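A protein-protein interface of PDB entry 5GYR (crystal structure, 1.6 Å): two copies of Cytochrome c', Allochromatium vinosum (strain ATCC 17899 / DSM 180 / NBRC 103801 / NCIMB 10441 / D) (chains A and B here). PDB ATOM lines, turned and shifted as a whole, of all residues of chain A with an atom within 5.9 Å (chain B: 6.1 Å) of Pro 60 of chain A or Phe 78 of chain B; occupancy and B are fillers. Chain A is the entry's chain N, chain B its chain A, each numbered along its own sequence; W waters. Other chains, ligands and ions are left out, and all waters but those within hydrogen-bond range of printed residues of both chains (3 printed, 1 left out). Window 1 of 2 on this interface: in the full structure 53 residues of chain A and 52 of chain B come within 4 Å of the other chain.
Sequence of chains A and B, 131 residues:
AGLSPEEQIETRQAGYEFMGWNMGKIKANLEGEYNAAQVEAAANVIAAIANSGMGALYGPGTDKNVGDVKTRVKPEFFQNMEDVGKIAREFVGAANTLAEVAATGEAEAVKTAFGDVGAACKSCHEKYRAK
OE1 of Glu 82 of chain B is in hydrogen-bond range of N of Gly 55 of chain A (3.1 Å). The backbone carbonyl oxygen (O) of Pro 60 of chain B lies within hydrogen-bond range of the backbone NH (N) of Gly 61 of chain A.
The side-chain amide nitrogen (NE2) of Gln 79 of chain B sits close to the backbone carbonyl oxygen (O) of Glu 76 of chain B (3.4 Å).
Among the printed residues, merely in contact across the chains: Pro 60 of chain A with Pro 60 of chain B (3.1 Å), Met 81 of chain A with Glu 82 of chain B (3.2 Å), Pro 60 of chain A with Asp 63 of chain B (3.3 Å), Gly 55 of chain A with Met 81 of chain B (3.4 Å), Pro 60 of chain A with Phe 78 of chain B (3.5 Å), Ala 56 of chain A with Gln 79 of chain B (3.5 Å), Asp 63 of chain A with Pro 60 of chain B (3.6 Å), Ala 56 of chain A with Met 81 of chain B (3.7 Å) and Met 81 of chain A with Met 81 of chain B (3.8 Å).
Printed residues of chain B within 4 Å of Pro 60 of chain A: Pro 60 (3.1 Å), Asp 63 (3.3 Å) and Phe 78 (3.5 Å). Of the printed residues of chain B, Gly 61 of chain A touches Pro 60 (2.9 Å). Of the printed residues of chain A, Pro 60 of chain B touches Pro 60, Gly 61 and Asp 63. Printed residues of chain A within 4 Å of Asp 63 of chain B: Pro 60. Of chain A, only Pro 60 comes within 4 Å of Phe 78 of chain B. The nearest printed residue of chain A that does not touch Asp 63 of chain B is Gly 61 of chain A (4.9 Å).
Hydrophobic or aromatic side chains of chain A within 4 Å of the printed part of chain B: Ala 56, Pro 60 and Met 81. Printed residues of chain B that touch a printed residue of chain A: Pro 60, Asp 63, Phe 78, Gln 79, Met 81 and Glu 82. Hydrophobic or aromatic side chains of chain B within 4 Å of the printed part of chain A: Pro 60, Phe 78 and Met 81. Among the printed residues, 11 pairs touch across the chains. Among the printed residues, no Asp or Glu carboxylate lies within 4 Å of a Lys or Arg side-chain nitrogen of the other chain.
Pro 60 of chain A touches its own counterpart, Pro 60 of chain B. Pro 60 of chain A touches Asp 63 of chain B, and with the chains exchanged Asp 63 of chain A touches Pro 60 of chain B. Gly 61 of chain A touches Pro 60 of chain B, but with the chains exchanged Pro 60 of chain A does not touch Gly 61 of chain B (5.1 Å). Met 81 of chain A touches its own counterpart, Met 81 of chain B. Positions printed for both chains: 58, 59, 60, 61, 62, 63 and 81. Of the 11 pairs that touch across the chains among the printed residues, 4 have their exchanged pair printed and touching as well.
Water W3 lies within hydrogen-bond range of the side-chain carboxylate (OD1) of Asp 63 of chain B (2.6 Å), the backbone carbonyl oxygen (O) of Pro 60 of chain B (2.8 Å) and the backbone NH (N) of Gly 61 of chain A (3.4 Å). Water W1 bridges the backbone carbonyl oxygen of Tyr 58 of chain B (3.0 Å) and the side-chain sulfur of Met 81 of chain A (3.5 Å). Water W2 lies within hydrogen-bond range of the backbone carbonyl oxygen of Tyr 58 of chain A (3.1 Å) and the side-chain sulfur of Met 81 of chain B (3.6 Å).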
ATOM      1  N   PRO A   5      -3.536  -1.484 -34.447  1.00  0.00           N
ATOM      2  CA  PRO A   5      -2.882  -0.624 -35.417  1.00  0.00           C
ATOM      3  C   PRO A   5      -3.491  -0.712 -36.818  1.00  0.00           C
ATOM      4  O   PRO A   5      -3.679   0.306 -37.482  1.00  0.00           O
ATOM      5  CB  PRO A   5      -1.444  -1.145 -35.427  1.00  0.00           C
ATOM      6  CG  PRO A   5      -1.248  -1.690 -34.063  1.00  0.00           C
ATOM      7  CD  PRO A   5      -2.572  -2.262 -33.651  1.00  0.00           C
ATOM      8  N   GLN A   8      -6.741   1.123 -36.815  1.00  0.00           N
ATOM      9  CA  GLN A   8      -6.520   2.573 -36.776  1.00  0.00           C
ATOM     10  C   GLN A   8      -6.227   3.133 -38.153  1.00  0.00           C
ATOM     11  O   GLN A   8      -6.766   4.166 -38.527  1.00  0.00           O
ATOM     12  CB  GLN A   8      -5.372   2.918 -35.834  1.00  0.00           C
ATOM     13  CG  GLN A   8      -5.690   2.665 -34.379  1.00  0.00           C
ATOM     14  CD  GLN A   8      -4.512   2.949 -33.473  1.00  0.00           C
ATOM     15  OE1 GLN A   8      -3.878   3.988 -33.572  1.00  0.00           O
ATOM     16  NE2 GLN A   8      -4.202   2.019 -32.599  1.00  0.00           N
ATOM     17  N   GLY A  55      -6.541  12.025 -34.195  1.00  0.00           N
ATOM     18  CA  GLY A  55      -5.247  11.809 -33.573  1.00  0.00           C
ATOM     19  C   GLY A  55      -5.189  10.481 -32.837  1.00  0.00           C
ATOM     20  O   GLY A  55      -4.140   9.855 -32.786  1.00  0.00           O
ATOM     21  N   ALA A  56      -6.328  10.047 -32.298  1.00  0.00           N
ATOM     22  CA  ALA A  56      -6.433   8.752 -31.616  1.00  0.00           C
ATOM     23  C   ALA A  56      -6.231   7.575 -32.564  1.00  0.00           C
ATOM     24  O   ALA A  56      -6.006   6.466 -32.096  1.00  0.00           O
ATOM     25  CB  ALA A  56      -7.786   8.624 -30.941  1.00  0.00           C
ATOM     26  N   TYR A  58      -3.711   7.596 -34.778  1.00  0.00           N
ATOM     27  CA  TYR A  58      -2.289   7.666 -35.124  1.00  0.00           C
ATOM     28  C   TYR A  58      -1.447   7.149 -33.966  1.00  0.00           C
ATOM     29  O   TYR A  58      -0.444   7.748 -33.548  1.00  0.00           O
ATOM     30  CB  TYR A  58      -1.895   9.087 -35.506  1.00  0.00           C
ATOM     31  CG  TYR A  58      -2.314   9.453 -36.901  1.00  0.00           C
ATOM     32  CD1 TYR A  58      -1.528   9.105 -37.992  1.00  0.00           C
ATOM     33  CD2 TYR A  58      -3.504  10.116 -37.134  1.00  0.00           C
ATOM     34  CE1 TYR A  58      -1.904   9.419 -39.282  1.00  0.00           C
ATOM     35  CE2 TYR A  58      -3.884  10.449 -38.430  1.00  0.00           C
ATOM     36  CZ  TYR A  58      -3.085  10.104 -39.495  1.00  0.00           C
ATOM     37  OH  TYR A  58      -3.467  10.426 -40.772  1.00  0.00           O
ATOM     38  N   GLY A  59      -1.865   5.991 -33.464  1.00  0.00           N
ATOM     39  CA  GLY A  59      -1.222   5.362 -32.321  1.00  0.00           C
ATOM     40  C   GLY A  59       0.080   4.690 -32.677  1.00  0.00           C
ATOM     41  O   GLY A  59       0.477   4.644 -33.849  1.00  0.00           O
ATOM     42  N   PRO A  60       0.759   4.152 -31.656  1.00  0.00           N
ATOM     43  CA  PRO A  60       1.997   3.436 -31.857  1.00  0.00           C
ATOM     44  C   PRO A  60       1.781   2.281 -32.794  1.00  0.00           C
ATOM     45  O   PRO A  60       0.757   1.637 -32.715  1.00  0.00           O
ATOM     46  CB  PRO A  60       2.326   2.856 -30.492  1.00  0.00           C
ATOM     47  CG  PRO A  60       1.414   3.461 -29.514  1.00  0.00           C
ATOM     48  CD  PRO A  60       0.400   4.286 -30.239  1.00  0.00           C
ATOM     49  N   GLY A  61       2.755   2.006 -33.642  1.00  0.00           N
ATOM     50  CA  GLY A  61       2.685   0.878 -34.542  1.00  0.00           C
ATOM     51  C   GLY A  61       1.920   1.160 -35.814  1.00  0.00           C
ATOM     52  O   GLY A  61       1.746   0.259 -36.602  1.00  0.00           O
ATOM     53  N   THR A  62       1.445   2.391 -36.012  1.00  0.00           N
ATOM     54  CA  THR A  62       0.710   2.742 -37.235  1.00  0.00           C
ATOM     55  C   THR A  62       1.528   3.570 -38.223  1.00  0.00           C
ATOM     56  O   THR A  62       0.970   4.159 -39.148  1.00  0.00           O
ATOM     57  CB  THR A  62      -0.594   3.518 -36.926  1.00  0.00           C
ATOM     58  OG1 THR A  62      -0.282   4.832 -36.442  1.00  0.00           O
ATOM     59  CG2 THR A  62      -1.427   2.789 -35.907  1.00  0.00           C
ATOM     60  N   ASP A  63       2.838   3.616 -38.024  1.00  0.00           N
ATOM     61  CA  ASP A  63       3.734   4.359 -38.900  1.00  0.00           C
ATOM     62  C   ASP A  63       4.199   3.553 -40.114  1.00  0.00           C
ATOM     63  O   ASP A  63       4.803   4.104 -41.025  1.00  0.00           O
ATOM     64  CB  ASP A  63       4.943   4.873 -38.114  1.00  0.00           C
ATOM     65  CG  ASP A  63       5.766   3.755 -37.501  1.00  0.00           C
ATOM     66  OD1 ASP A  63       5.176   2.793 -36.968  1.00  0.00           O
ATOM     67  OD2 ASP A  63       7.003   3.844 -37.546  1.00  0.00           O
ATOM     68  N   MET A  81       2.098  15.668 -32.792  1.00  0.00           N
ATOM     69  CA  MET A  81       1.083  15.296 -31.805  1.00  0.00           C
ATOM     70  C   MET A  81       1.447  15.644 -30.359  1.00  0.00           C
ATOM     71  O   MET A  81       2.612  15.600 -29.976  1.00  0.00           O
ATOM     72  CB  MET A  81       0.752  13.793 -31.948  1.00  0.00           C
ATOM     73  CG  MET A  81       0.207  13.459 -33.333  1.00  0.00           C
ATOM     74  SD  MET A  81       0.233  11.720 -33.713  1.00  0.00           S
ATOM     75  CE  MET A  81      -1.005  11.169 -32.551  1.00  0.00           C
ATOM     76  N   ARG B  12      12.091  11.695 -22.763  1.00  0.00           N
ATOM     77  CA  ARG B  12      10.931  11.943 -21.932  1.00  0.00           C
ATOM     78  C   ARG B  12      11.211  11.520 -20.496  1.00  0.00           C
ATOM     79  O   ARG B  12      10.872  12.226 -19.570  1.00  0.00           O
ATOM     80  CB  ARG B  12       9.661  11.320 -22.511  1.00  0.00           C
ATOM     81  CG  ARG B  12       9.553   9.811 -22.412  1.00  0.00           C
ATOM     82  CD  ARG B  12       8.606   9.299 -23.487  1.00  0.00           C
ATOM     83  NE  ARG B  12       8.301   7.886 -23.332  1.00  0.00           N
ATOM     84  CZ  ARG B  12       7.732   7.141 -24.273  1.00  0.00           C
ATOM     85  NH1 ARG B  12       7.499   5.861 -24.047  1.00  0.00           N
ATOM     86  NH2 ARG B  12       7.417   7.661 -25.440  1.00  0.00           N
ATOM     87  N   TYR B  58       6.500  10.999 -27.794  1.00  0.00           N
ATOM     88  CA  TYR B  58       5.627   9.834 -27.713  1.00  0.00           C
ATOM     89  C   TYR B  58       5.268   9.349 -29.109  1.00  0.00           C
ATOM     90  O   TYR B  58       4.102   9.124 -29.435  1.00  0.00           O
ATOM     91  CB  TYR B  58       4.376  10.145 -26.876  1.00  0.00           C
ATOM     92  CG  TYR B  58       4.627  10.125 -25.385  1.00  0.00           C
ATOM     93  CD1 TYR B  58       4.614   8.921 -24.687  1.00  0.00           C
ATOM     94  CD2 TYR B  58       4.931  11.290 -24.683  1.00  0.00           C
ATOM     95  CE1 TYR B  58       4.831   8.883 -23.333  1.00  0.00           C
ATOM     96  CE2 TYR B  58       5.171  11.253 -23.319  1.00  0.00           C
ATOM     97  CZ  TYR B  58       5.124  10.043 -22.648  1.00  0.00           C
ATOM     98  OH  TYR B  58       5.370   9.994 -21.297  1.00  0.00           O
ATOM     99  N   GLY B  59       6.293   9.208 -29.946  1.00  0.00           N
ATOM    100  CA  GLY B  59       6.136   8.797 -31.347  1.00  0.00           C
ATOM    101  C   GLY B  59       5.821   7.313 -31.468  1.00  0.00           C
ATOM    102  O   GLY B  59       5.854   6.609 -30.483  1.00  0.00           O
ATOM    103  N   PRO B  60       5.506   6.832 -32.686  1.00  0.00           N
ATOM    104  CA  PRO B  60       4.877   5.506 -32.916  1.00  0.00           C
ATOM    105  C   PRO B  60       5.641   4.221 -32.478  1.00  0.00           C
ATOM    106  O   PRO B  60       5.018   3.166 -32.234  1.00  0.00           O
ATOM    107  CB  PRO B  60       4.599   5.490 -34.441  1.00  0.00           C
ATOM    108  CG  PRO B  60       5.180   6.739 -35.002  1.00  0.00           C
ATOM    109  CD  PRO B  60       5.472   7.691 -33.882  1.00  0.00           C
ATOM    110  N   GLY B  61       6.966   4.300 -32.372  1.00  0.00           N
ATOM    111  CA  GLY B  61       7.767   3.138 -31.960  1.00  0.00           C
ATOM    112  C   GLY B  61       8.083   3.086 -30.478  1.00  0.00           C
ATOM    113  O   GLY B  61       8.914   2.281 -30.054  1.00  0.00           O
ATOM    114  N   THR B  62       7.424   3.930 -29.688  1.00  0.00           N
ATOM    115  CA  THR B  62       7.831   4.149 -28.289  1.00  0.00           C
ATOM    116  C   THR B  62       6.866   3.585 -27.244  1.00  0.00           C
ATOM    117  O   THR B  62       6.957   3.930 -26.077  1.00  0.00           O
ATOM    118  CB  THR B  62       8.022   5.652 -28.005  1.00  0.00           C
ATOM    119  OG1 THR B  62       6.759   6.309 -27.962  1.00  0.00           O
ATOM    120  CG2 THR B  62       8.892   6.286 -29.061  1.00  0.00           C
ATOM    121  N   ASP B  63       5.967   2.707 -27.669  1.00  0.00           N
ATOM    122  CA  ASP B  63       5.023   2.073 -26.747  1.00  0.00           C
ATOM    123  C   ASP B  63       5.594   0.822 -26.059  1.00  0.00           C
ATOM    124  O   ASP B  63       4.967   0.289 -25.149  1.00  0.00           O
ATOM    125  CB  ASP B  63       3.724   1.715 -27.477  1.00  0.00           C
ATOM    126  CG  ASP B  63       3.945   0.739 -28.619  1.00  0.00           C
ATOM    127  OD1 ASP B  63       4.916   0.928 -29.390  1.00  0.00           O
ATOM    128  OD2 ASP B  63       3.117  -0.163 -28.791  1.00  0.00           O
ATOM    129  N   VAL B  73       5.383   3.349 -20.048  1.00  0.00           N
ATOM    130  CA  VAL B  73       4.134   3.900 -20.559  1.00  0.00           C
ATOM    131  C   VAL B  73       3.125   2.788 -20.804  1.00  0.00           C
ATOM    132  O   VAL B  73       3.482   1.694 -21.252  1.00  0.00           O
ATOM    133  CB  VAL B  73       4.341   4.736 -21.835  1.00  0.00           C
ATOM    134  CG1 VAL B  73       4.701   3.851 -23.024  1.00  0.00           C
ATOM    135  CG2 VAL B  73       3.100   5.574 -22.115  1.00  0.00           C
ATOM    136  N   LYS B  74       1.869   3.069 -20.468  1.00  0.00           N
ATOM    137  CA  LYS B  74       0.759   2.174 -20.795  1.00  0.00           C
ATOM    138  C   LYS B  74       0.176   2.536 -22.153  1.00  0.00           C
ATOM    139  O   LYS B  74       0.109   3.705 -22.507  1.00  0.00           O
ATOM    140  CB  LYS B  74      -0.323   2.272 -19.733  1.00  0.00           C
ATOM    141  CG  LYS B  74       0.118   1.712 -18.397  1.00  0.00           C
ATOM    142  CD  LYS B  74      -0.898   2.014 -17.322  1.00  0.00           C
ATOM    143  CE  LYS B  74      -2.066   1.054 -17.369  1.00  0.00           C
ATOM    144  NZ  LYS B  74      -2.213   0.372 -16.054  1.00  0.00           N
ATOM    145  N   PRO B  75      -0.267   1.543 -22.923  1.00  0.00           N
ATOM    146  CA  PRO B  75      -0.702   1.807 -24.301  1.00  0.00           C
ATOM    147  C   PRO B  75      -1.863   2.810 -24.375  1.00  0.00           C
ATOM    148  O   PRO B  75      -1.970   3.540 -25.349  1.00  0.00           O
ATOM    149  CB  PRO B  75      -1.125   0.419 -24.834  1.00  0.00           C
ATOM    150  CG  PRO B  75      -0.930  -0.557 -23.724  1.00  0.00           C
ATOM    151  CD  PRO B  75      -0.215   0.103 -22.595  1.00  0.00           C
ATOM    152  N   GLU B  76      -2.686   2.843 -23.326  1.00  0.00           N
ATOM    153  CA  GLU B  76      -3.845   3.741 -23.234  1.00  0.00           C
ATOM    154  C   GLU B  76      -3.484   5.208 -23.348  1.00  0.00           C
ATOM    155  O   GLU B  76      -4.327   6.033 -23.679  1.00  0.00           O
ATOM    156  CB  GLU B  76      -4.583   3.544 -21.902  1.00  0.00           C
ATOM    157  CG  GLU B  76      -5.339   2.226 -21.782  1.00  0.00           C
ATOM    158  CD  GLU B  76      -4.525   1.058 -21.263  1.00  0.00           C
ATOM    159  OE1 GLU B  76      -3.280   1.124 -21.221  1.00  0.00           O
ATOM    160  OE2 GLU B  76      -5.168   0.050 -20.907  1.00  0.00           O
ATOM    161  N   PHE B  77      -2.250   5.541 -23.009  1.00  0.00           N
ATOM    162  CA  PHE B  77      -1.804   6.922 -23.017  1.00  0.00           C
ATOM    163  C   PHE B  77      -1.926   7.570 -24.387  1.00  0.00           C
ATOM    164  O   PHE B  77      -2.420   8.702 -24.510  1.00  0.00           O
ATOM    165  CB  PHE B  77      -0.344   6.968 -22.577  1.00  0.00           C
ATOM    166  CG  PHE B  77       0.190   8.372 -22.470  1.00  0.00           C
ATOM    167  CD1 PHE B  77      -0.241   9.220 -21.449  1.00  0.00           C
ATOM    168  CD2 PHE B  77       1.088   8.851 -23.395  1.00  0.00           C
ATOM    169  CE1 PHE B  77       0.232  10.520 -21.355  1.00  0.00           C
ATOM    170  CE2 PHE B  77       1.572  10.143 -23.303  1.00  0.00           C
ATOM    171  CZ  PHE B  77       1.144  10.979 -22.283  1.00  0.00           C
ATOM    172  N   PHE B  78      -1.517   6.832 -25.415  1.00  0.00           N
ATOM    173  CA  PHE B  78      -1.367   7.373 -26.759  1.00  0.00           C
ATOM    174  C   PHE B  78      -2.659   7.885 -27.405  1.00  0.00           C
ATOM    175  O   PHE B  78      -2.641   8.822 -28.201  1.00  0.00           O
ATOM    176  CB  PHE B  78      -0.713   6.337 -27.655  1.00  0.00           C
ATOM    177  CG  PHE B  78       0.696   6.045 -27.276  1.00  0.00           C
ATOM    178  CD1 PHE B  78       1.730   6.803 -27.807  1.00  0.00           C
ATOM    179  CD2 PHE B  78       1.001   5.057 -26.362  1.00  0.00           C
ATOM    180  CE1 PHE B  78       3.041   6.543 -27.442  1.00  0.00           C
ATOM    181  CE2 PHE B  78       2.317   4.801 -25.992  1.00  0.00           C
ATOM    182  CZ  PHE B  78       3.334   5.540 -26.544  1.00  0.00           C
ATOM    183  N   GLN B  79      -3.786   7.302 -27.049  1.00  0.00           N
ATOM    184  CA  GLN B  79      -5.047   7.695 -27.704  1.00  0.00           C
ATOM    185  C   GLN B  79      -5.514   9.098 -27.311  1.00  0.00           C
ATOM    186  O   GLN B  79      -6.412   9.664 -27.932  1.00  0.00           O
ATOM    187  CB  GLN B  79      -6.156   6.678 -27.423  1.00  0.00           C
ATOM    188  CG  GLN B  79      -6.551   6.583 -25.974  1.00  0.00           C
ATOM    189  CD  GLN B  79      -7.496   5.433 -25.730  1.00  0.00           C
ATOM    190  OE1 GLN B  79      -8.436   5.224 -26.490  1.00  0.00           O
ATOM    191  NE2 GLN B  79      -7.260   4.687 -24.673  1.00  0.00           N
ATOM    192  N   ASN B  80      -4.905   9.642 -26.263  1.00  0.00           N
ATOM    193  CA  ASN B  80      -5.215  11.019 -25.846  1.00  0.00           C
ATOM    194  C   ASN B  80      -4.478  12.123 -26.596  1.00  0.00           C
ATOM    195  O   ASN B  80      -4.682  13.307 -26.293  1.00  0.00           O
ATOM    196  CB  ASN B  80      -4.946  11.219 -24.365  1.00  0.00           C
ATOM    197  CG  ASN B  80      -5.743  10.278 -23.514  1.00  0.00           C
ATOM    198  OD1 ASN B  80      -6.913  10.517 -23.256  1.00  0.00           O
ATOM    199  ND2 ASN B  80      -5.135   9.157 -23.129  1.00  0.00           N
ATOM    200  N   MET B  81      -3.583  11.739 -27.505  1.00  0.00           N
ATOM    201  CA  MET B  81      -2.835  12.655 -28.352  1.00  0.00           C
ATOM    202  C   MET B  81      -3.593  13.098 -29.582  1.00  0.00           C
ATOM    203  O   MET B  81      -4.376  12.339 -30.163  1.00  0.00           O
ATOM    204  CB  MET B  81      -1.479  12.039 -28.740  1.00  0.00           C
ATOM    205  CG  MET B  81      -0.626  11.757 -27.505  1.00  0.00           C
ATOM    206  SD  MET B  81       0.737  10.665 -27.828  1.00  0.00           S
ATOM    207  CE  MET B  81       1.717  11.767 -28.858  1.00  0.00           C
ATOM    208  N   GLU B  82      -3.340  14.348 -29.961  1.00  0.00           N
ATOM    209  CA  GLU B  82      -3.887  14.948 -31.151  1.00  0.00           C
ATOM    210  C   GLU B  82      -2.832  15.747 -31.881  1.00  0.00           C
ATOM    211  O   GLU B  82      -1.898  16.273 -31.275  1.00  0.00           O
ATOM    212  CB  GLU B  82      -5.055  15.846 -30.783  1.00  0.00           C
ATOM    213  CG  GLU B  82      -5.838  16.370 -31.935  1.00  0.00           C
ATOM    214  CD  GLU B  82      -6.378  15.273 -32.813  1.00  0.00           C
ATOM    215  OE1 GLU B  82      -7.185  14.449 -32.348  1.00  0.00           O
ATOM    216  OE2 GLU B  82      -5.964  15.231 -33.978  1.00  0.00           O
HETATM  217  O   HOH W   1       2.658   9.826 -31.965  1.00  0.00           O
HETATM  218  O   HOH W   2       0.195   8.363 -30.549  1.00  0.00           O
HETATM  219  O   HOH W   3       5.242   0.387 -31.954  1.00  0.00           O
